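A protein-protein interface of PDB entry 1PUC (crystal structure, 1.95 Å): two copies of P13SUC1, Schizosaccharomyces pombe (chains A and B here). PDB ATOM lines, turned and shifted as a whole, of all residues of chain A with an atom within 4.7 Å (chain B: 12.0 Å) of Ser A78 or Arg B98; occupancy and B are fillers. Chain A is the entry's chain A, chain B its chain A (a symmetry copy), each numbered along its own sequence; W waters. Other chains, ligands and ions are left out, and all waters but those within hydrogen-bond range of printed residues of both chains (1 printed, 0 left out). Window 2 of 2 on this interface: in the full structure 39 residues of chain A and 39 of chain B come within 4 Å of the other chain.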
ATOM      1  N   ARG A  29      22.157 -21.246 -34.482  1.00  0.00           N
ATOM      2  CA  ARG A  29      21.931 -20.037 -33.713  1.00  0.00           C
ATOM      3  C   ARG A  29      21.009 -19.074 -34.458  1.00  0.00           C
ATOM      4  O   ARG A  29      21.018 -19.019 -35.690  1.00  0.00           O
ATOM      5  CB  ARG A  29      23.271 -19.351 -33.425  1.00  0.00           C
ATOM      6  CG  ARG A  29      24.331 -20.261 -32.809  1.00  0.00           C
ATOM      7  CD  ARG A  29      25.664 -19.555 -32.734  1.00  0.00           C
ATOM      8  NE  ARG A  29      26.009 -18.946 -34.014  1.00  0.00           N
ATOM      9  CZ  ARG A  29      26.951 -18.020 -34.179  1.00  0.00           C
ATOM     10  NH1 ARG A  29      27.660 -17.588 -33.143  1.00  0.00           N
ATOM     11  NH2 ARG A  29      27.145 -17.480 -35.374  1.00  0.00           N
ATOM     12  N   GLU A  34      20.025  -7.627 -29.452  1.00  0.00           N
ATOM     13  CA  GLU A  34      21.141  -7.725 -28.528  1.00  0.00           C
ATOM     14  C   GLU A  34      21.585  -9.113 -28.083  1.00  0.00           C
ATOM     15  O   GLU A  34      22.592  -9.242 -27.386  1.00  0.00           O
ATOM     16  CB  GLU A  34      20.867  -6.848 -27.303  1.00  0.00           C
ATOM     17  CG  GLU A  34      19.546  -7.135 -26.602  1.00  0.00           C
ATOM     18  CD  GLU A  34      19.387  -6.351 -25.306  1.00  0.00           C
ATOM     19  OE1 GLU A  34      20.183  -6.572 -24.362  1.00  0.00           O
ATOM     20  OE2 GLU A  34      18.461  -5.515 -25.227  1.00  0.00           O
ATOM     21  N   TYR A  35      20.867 -10.149 -28.498  1.00  0.00           N
ATOM     22  CA  TYR A  35      21.213 -11.510 -28.097  1.00  0.00           C
ATOM     23  C   TYR A  35      21.178 -12.550 -29.191  1.00  0.00           C
ATOM     24  O   TYR A  35      20.416 -12.430 -30.151  1.00  0.00           O
ATOM     25  CB  TYR A  35      20.266 -12.000 -26.992  1.00  0.00           C
ATOM     26  CG  TYR A  35      20.483 -11.356 -25.642  1.00  0.00           C
ATOM     27  CD1 TYR A  35      21.448 -11.838 -24.767  1.00  0.00           C
ATOM     28  CD2 TYR A  35      19.715 -10.272 -25.238  1.00  0.00           C
ATOM     29  CE1 TYR A  35      21.646 -11.255 -23.531  1.00  0.00           C
ATOM     30  CE2 TYR A  35      19.906  -9.682 -24.003  1.00  0.00           C
ATOM     31  CZ  TYR A  35      20.872 -10.177 -23.154  1.00  0.00           C
ATOM     32  OH  TYR A  35      21.065  -9.590 -21.924  1.00  0.00           O
ATOM     33  N   GLU A  36      22.032 -13.536 -28.973  1.00  0.00           N
ATOM     34  CA  GLU A  36      22.103 -14.729 -29.778  1.00  0.00           C
ATOM     35  C   GLU A  36      21.398 -15.827 -29.005  1.00  0.00           C
ATOM     36  O   GLU A  36      21.452 -15.859 -27.777  1.00  0.00           O
ATOM     37  CB  GLU A  36      23.563 -15.124 -30.033  1.00  0.00           C
ATOM     38  CG  GLU A  36      24.253 -14.396 -31.174  1.00  0.00           C
ATOM     39  CD  GLU A  36      25.527 -15.102 -31.602  1.00  0.00           C
ATOM     40  OE1 GLU A  36      25.434 -16.055 -32.406  1.00  0.00           O
ATOM     41  OE2 GLU A  36      26.616 -14.711 -31.131  1.00  0.00           O
ATOM     42  N   ARG A  71      27.874 -27.755 -18.448  1.00  0.00           N
ATOM     43  CA  ARG A  71      29.032 -28.316 -19.138  1.00  0.00           C
ATOM     44  C   ARG A  71      29.300 -29.672 -18.485  1.00  0.00           C
ATOM     45  O   ARG A  71      29.620 -30.650 -19.166  1.00  0.00           O
ATOM     46  CB  ARG A  71      30.255 -27.395 -19.026  1.00  0.00           C
ATOM     47  CG  ARG A  71      30.106 -26.085 -19.793  1.00  0.00           C
ATOM     48  CD  ARG A  71      31.433 -25.353 -19.992  1.00  0.00           C
ATOM     49  NE  ARG A  71      31.267 -24.081 -20.702  1.00  0.00           N
ATOM     50  CZ  ARG A  71      31.314 -23.932 -22.027  1.00  0.00           C
ATOM     51  NH1 ARG A  71      31.525 -24.982 -22.814  1.00  0.00           N
ATOM     52  NH2 ARG A  71      31.136 -22.732 -22.569  1.00  0.00           N
ATOM     53  N   GLN A  77      29.482 -26.200 -25.719  1.00  0.00           N
ATOM     54  CA  GLN A  77      29.184 -25.042 -26.555  1.00  0.00           C
ATOM     55  C   GLN A  77      30.364 -24.096 -26.421  1.00  0.00           C
ATOM     56  O   GLN A  77      31.237 -24.308 -25.579  1.00  0.00           O
ATOM     57  CB  GLN A  77      27.944 -24.316 -26.040  1.00  0.00           C
ATOM     58  CG  GLN A  77      26.736 -25.190 -25.877  1.00  0.00           C
ATOM     59  CD  GLN A  77      25.503 -24.386 -25.587  1.00  0.00           C
ATOM     60  OE1 GLN A  77      24.816 -23.944 -26.497  1.00  0.00           O
ATOM     61  NE2 GLN A  77      25.213 -24.185 -24.315  1.00  0.00           N
ATOM     62  N   SER A  78      30.383 -23.047 -27.232  1.00  0.00           N
ATOM     63  CA  SER A  78      31.448 -22.059 -27.161  1.00  0.00           C
ATOM     64  C   SER A  78      31.270 -21.202 -25.900  1.00  0.00           C
ATOM     65  O   SER A  78      30.524 -21.567 -24.988  1.00  0.00           O
ATOM     66  CB  SER A  78      31.469 -21.202 -28.437  1.00  0.00           C
ATOM     67  OG  SER A  78      30.167 -20.794 -28.825  1.00  0.00           O
ATOM     68  N   LEU A  79      31.939 -20.061 -25.845  1.00  0.00           N
ATOM     69  CA  LEU A  79      31.844 -19.198 -24.671  1.00  0.00           C
ATOM     70  C   LEU A  79      30.703 -18.175 -24.737  1.00  0.00           C
ATOM     71  O   LEU A  79      30.268 -17.786 -25.825  1.00  0.00           O
ATOM     72  CB  LEU A  79      33.160 -18.444 -24.480  1.00  0.00           C
ATOM     73  CG  LEU A  79      34.444 -19.267 -24.537  1.00  0.00           C
ATOM     74  CD1 LEU A  79      35.648 -18.363 -24.304  1.00  0.00           C
ATOM     75  CD2 LEU A  79      34.379 -20.351 -23.492  1.00  0.00           C
ATOM     76  N   GLY A  80      30.226 -17.751 -23.564  1.00  0.00           N
ATOM     77  CA  GLY A  80      29.187 -16.737 -23.480  1.00  0.00           C
ATOM     78  C   GLY A  80      27.767 -17.177 -23.206  1.00  0.00           C
ATOM     79  O   GLY A  80      26.972 -16.412 -22.668  1.00  0.00           O
ATOM     80  N   TRP A  81      27.441 -18.406 -23.575  1.00  0.00           N
ATOM     81  CA  TRP A  81      26.096 -18.932 -23.386  1.00  0.00           C
ATOM     82  C   TRP A  81      25.639 -19.038 -21.937  1.00  0.00           C
ATOM     83  O   TRP A  81      26.391 -19.445 -21.052  1.00  0.00           O
ATOM     84  CB  TRP A  81      25.980 -20.294 -24.065  1.00  0.00           C
ATOM     85  CG  TRP A  81      26.306 -20.249 -25.519  1.00  0.00           C
ATOM     86  CD1 TRP A  81      27.478 -20.632 -26.117  1.00  0.00           C
ATOM     87  CD2 TRP A  81      25.452 -19.784 -26.568  1.00  0.00           C
ATOM     88  NE1 TRP A  81      27.401 -20.433 -27.478  1.00  0.00           N
ATOM     89  CE2 TRP A  81      26.170 -19.913 -27.782  1.00  0.00           C
ATOM     90  CE3 TRP A  81      24.150 -19.266 -26.603  1.00  0.00           C
ATOM     91  CZ2 TRP A  81      25.627 -19.543 -29.016  1.00  0.00           C
ATOM     92  CZ3 TRP A  81      23.613 -18.897 -27.833  1.00  0.00           C
ATOM     93  CH2 TRP A  81      24.351 -19.037 -29.020  1.00  0.00           C
ATOM     94  N   LEU B  94      16.623 -27.403 -23.649  1.00  0.00           N
ATOM     95  CA  LEU B  94      17.213 -26.336 -22.852  1.00  0.00           C
ATOM     96  C   LEU B  94      17.477 -25.109 -23.728  1.00  0.00           C
ATOM     97  O   LEU B  94      17.937 -25.225 -24.874  1.00  0.00           O
ATOM     98  CB  LEU B  94      18.524 -26.816 -22.222  1.00  0.00           C
ATOM     99  CG  LEU B  94      18.568 -28.185 -21.528  1.00  0.00           C
ATOM    100  CD1 LEU B  94      19.880 -28.334 -20.787  1.00  0.00           C
ATOM    101  CD2 LEU B  94      17.406 -28.321 -20.568  1.00  0.00           C
ATOM    102  N   LEU B  95      17.232 -23.936 -23.163  1.00  0.00           N
ATOM    103  CA  LEU B  95      17.409 -22.694 -23.895  1.00  0.00           C
ATOM    104  C   LEU B  95      18.628 -21.933 -23.401  1.00  0.00           C
ATOM    105  O   LEU B  95      18.869 -21.853 -22.194  1.00  0.00           O
ATOM    106  CB  LEU B  95      16.155 -21.832 -23.734  1.00  0.00           C
ATOM    107  CG  LEU B  95      14.805 -22.502 -23.995  1.00  0.00           C
ATOM    108  CD1 LEU B  95      13.699 -21.492 -23.673  1.00  0.00           C
ATOM    109  CD2 LEU B  95      14.688 -23.004 -25.439  1.00  0.00           C
ATOM    110  N   PHE B  96      19.396 -21.384 -24.332  1.00  0.00           N
ATOM    111  CA  PHE B  96      20.598 -20.625 -24.001  1.00  0.00           C
ATOM    112  C   PHE B  96      20.607 -19.358 -24.823  1.00  0.00           C
ATOM    113  O   PHE B  96      19.986 -19.292 -25.890  1.00  0.00           O
ATOM    114  CB  PHE B  96      21.866 -21.423 -24.353  1.00  0.00           C
ATOM    115  CG  PHE B  96      22.062 -22.650 -23.518  1.00  0.00           C
ATOM    116  CD1 PHE B  96      22.730 -22.577 -22.304  1.00  0.00           C
ATOM    117  CD2 PHE B  96      21.556 -23.870 -23.927  1.00  0.00           C
ATOM    118  CE1 PHE B  96      22.888 -23.704 -21.512  1.00  0.00           C
ATOM    119  CE2 PHE B  96      21.710 -24.999 -23.142  1.00  0.00           C
ATOM    120  CZ  PHE B  96      22.375 -24.915 -21.935  1.00  0.00           C
ATOM    121  N   LYS B  97      21.312 -18.355 -24.324  1.00  0.00           N
ATOM    122  CA  LYS B  97      21.442 -17.092 -25.036  1.00  0.00           C
ATOM    123  C   LYS B  97      22.720 -16.427 -24.598  1.00  0.00           C
ATOM    124  O   LYS B  97      23.276 -16.779 -23.555  1.00  0.00           O
ATOM    125  CB  LYS B  97      20.257 -16.158 -24.756  1.00  0.00           C
ATOM    126  CG  LYS B  97      20.179 -15.611 -23.346  1.00  0.00           C
ATOM    127  CD  LYS B  97      18.939 -14.750 -23.218  1.00  0.00           C
ATOM    128  CE  LYS B  97      18.754 -14.244 -21.810  1.00  0.00           C
ATOM    129  NZ  LYS B  97      17.518 -13.423 -21.703  1.00  0.00           N
ATOM    130  N   ARG B  98      23.223 -15.520 -25.426  1.00  0.00           N
ATOM    131  CA  ARG B  98      24.428 -14.770 -25.088  1.00  0.00           C
ATOM    132  C   ARG B  98      24.365 -13.399 -25.752  1.00  0.00           C
ATOM    133  O   ARG B  98      23.761 -13.234 -26.819  1.00  0.00           O
ATOM    134  CB  ARG B  98      25.714 -15.512 -25.490  1.00  0.00           C
ATOM    135  CG  ARG B  98      25.926 -15.706 -26.969  1.00  0.00           C
ATOM    136  CD  ARG B  98      27.326 -16.237 -27.261  1.00  0.00           C
ATOM    137  NE  ARG B  98      27.479 -16.547 -28.682  1.00  0.00           N
ATOM    138  CZ  ARG B  98      28.515 -17.192 -29.212  1.00  0.00           C
ATOM    139  NH1 ARG B  98      29.514 -17.610 -28.449  1.00  0.00           N
ATOM    140  NH2 ARG B  98      28.548 -17.425 -30.516  1.00  0.00           N
ATOM    141  N   GLU B  99      24.957 -12.412 -25.096  1.00  0.00           N
ATOM    142  CA  GLU B  99      24.965 -11.055 -25.615  1.00  0.00           C
ATOM    143  C   GLU B  99      25.795 -10.945 -26.884  1.00  0.00           C
ATOM    144  O   GLU B  99      26.860 -11.555 -26.999  1.00  0.00           O
ATOM    145  CB  GLU B  99      25.516 -10.095 -24.562  1.00  0.00           C
ATOM    146  CG  GLU B  99      24.820 -10.187 -23.228  1.00  0.00           C
ATOM    147  CD  GLU B  99      25.067  -8.980 -22.367  1.00  0.00           C
ATOM    148  OE1 GLU B  99      24.466  -7.921 -22.661  1.00  0.00           O
ATOM    149  OE2 GLU B  99      25.855  -9.092 -21.400  1.00  0.00           O
ATOM    150  N   LYS B 100      25.290 -10.187 -27.845  1.00  0.00           N
ATOM    151  CA  LYS B 100      26.002  -9.973 -29.092  1.00  0.00           C
ATOM    152  C   LYS B 100      26.955  -8.801 -28.888  1.00  0.00           C
ATOM    153  O   LYS B 100      26.625  -7.846 -28.179  1.00  0.00           O
ATOM    154  CB  LYS B 100      25.026  -9.616 -30.213  1.00  0.00           C
ATOM    155  CG  LYS B 100      24.031 -10.691 -30.539  1.00  0.00           C
ATOM    156  CD  LYS B 100      23.019 -10.214 -31.567  1.00  0.00           C
ATOM    157  CE  LYS B 100      23.667  -9.929 -32.907  1.00  0.00           C
ATOM    158  NZ  LYS B 100      22.646  -9.548 -33.921  1.00  0.00           N
ATOM    159  N   ASP B 101      28.128  -8.870 -29.509  1.00  0.00           N
ATOM    160  CA  ASP B 101      29.110  -7.789 -29.421  1.00  0.00           C
ATOM    161  C   ASP B 101      29.455  -7.279 -30.814  1.00  0.00           C
ATOM    162  O   ASP B 101      28.714  -7.519 -31.770  1.00  0.00           O
ATOM    163  CB  ASP B 101      30.379  -8.252 -28.709  1.00  0.00           C
ATOM    164  CG  ASP B 101      30.413  -7.828 -27.264  1.00  0.00           C
ATOM    165  OD1 ASP B 101      30.468  -6.609 -27.012  1.00  0.00           O
ATOM    166  OD2 ASP B 101      30.379  -8.707 -26.381  1.00  0.00           O
HETATM  167  O   HOH W   1      28.445 -20.560 -31.485  1.00  0.00           O
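Among the printed residues, merely in contact across the chains: Glu A36 with Lys B97 (3.0 Å), Gly A80 with Arg B98 (3.2 Å), Tyr A35 with Arg B98 (3.3 Å), Tyr A35 with Glu B99 (3.4 Å), Glu A34 with Glu B99 (3.5 Å), Trp A81 with Arg B98 (3.5 Å), Trp A81 with Lys B97 (3.6 Å), Gln A77 with Phe B96 (3.6 Å), Tyr A35 with Lys B100 (3.7 Å), Glu A36 with Lys B100 (3.8 Å), Gly A80 with Lys B97 (3.8 Å) and Trp A81 with Phe B96 (3.9 Å).
The guanidinium group (NH1) of Arg A29 lies within salt-bridge range of the side-chain carboxylate (OE1) of Glu A36. NH1 of Arg A71 sits at hydrogen-bond distance from O of Gln A77 (2.9 Å). The guanidinium group (NH2) of Arg A71 is in hydrogen-bond range of the backbone carbonyl oxygen (O) of Ser A78 (2.8 Å). The indole nitrogen of Trp A81 sits at hydrogen-bond distance from the side-chain hydroxyl of Ser A78 (3.1 Å).
Water W1 lies within hydrogen-bond range of OG of Ser A78 (3.2 Å), NH2 of Arg B98 (3.3 Å) and NH1 of Arg A29 (3.5 Å).
Of the 10 printed residues of chain A, 9 touch a printed residue of chain B. Hydrophobic or aromatic side chains of chain A within 4 Å of the printed part of chain B: Tyr A35 and Trp A81. Along chain A the printed residues that touch a printed residue of chain B span positions 29 to 81. Hydrophobic or aromatic side chains of chain B within 4 Å of the printed part of chain A: Phe B96. Among the printed residues, 17 pairs touch across the chains. Among the printed residues, Asp or Glu carboxylates within 4 Å of a Lys or Arg side-chain nitrogen of the other chain: Glu A36 with Arg B98.
No position is printed for both chains.
Ser A78 touches just one residue of chain B: Arg B98. Arg B98 touches just these residues of chain A: Arg A29 (2.8 Å), Tyr A35 (3.3 Å), Glu A36 (2.8 Å), Ser A78 (3.3 Å), Leu A79 (2.7 Å), Gly A80 (3.2 Å) and Trp A81 (3.5 Å). Glu A36 touches just these residues of chain B: Lys B97, Arg B98 and Lys B100. Of chain B, only Phe B96 (3.6 Å) comes within 4 Å of Gln A77. Of the printed residues of chain B, Gly A80 touches Lys B97 (3.8 Å) and Arg B98 (3.2 Å). Of chain B, only Phe B96, Lys B97 and Arg B98 come within 4 Å of Trp A81. Printed residues of chain A within 4 Å of Glu B99: Glu A34 (3.5 Å) and Tyr A35 (3.4 Å). Of the printed residues of chain A, Lys B100 touches Glu A34, Tyr A35 and Glu A36. Printed residues of chain A within 4 Å of Phe B96: Gln A77 (3.6 Å) and Trp A81 (3.9 Å). Printed residues of chain A within 4 Å of Lys B97: Glu A36 (3.0 Å), Gly A80 (3.8 Å) and Trp A81 (3.6 Å). Leu B94 touches none of the printed residues of chain A. Leu B95 touches none of the printed residues of chain A. The nearest residue of chain A that does not touch Arg B98 is Glu A34 (4.2 Å).
The backbone carbonyl oxygen (O) of Glu A34 lies within hydrogen-bond range of the backbone NH (N) of Lys B100. The side-chain carboxylate of Glu A36 lies within salt-bridge range of the guanidinium group of Arg B98 (3.2 Å). OG of Ser A78 is in hydrogen-bond range of NH1 of Arg B98, at 3.3 Å. NH1 of Arg B98 lies within hydrogen-bond range of O of Leu A79, 2.7 Å away. NH1 of Arg A29 lies close to NH2 of Arg B98, 2.8 Å away.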
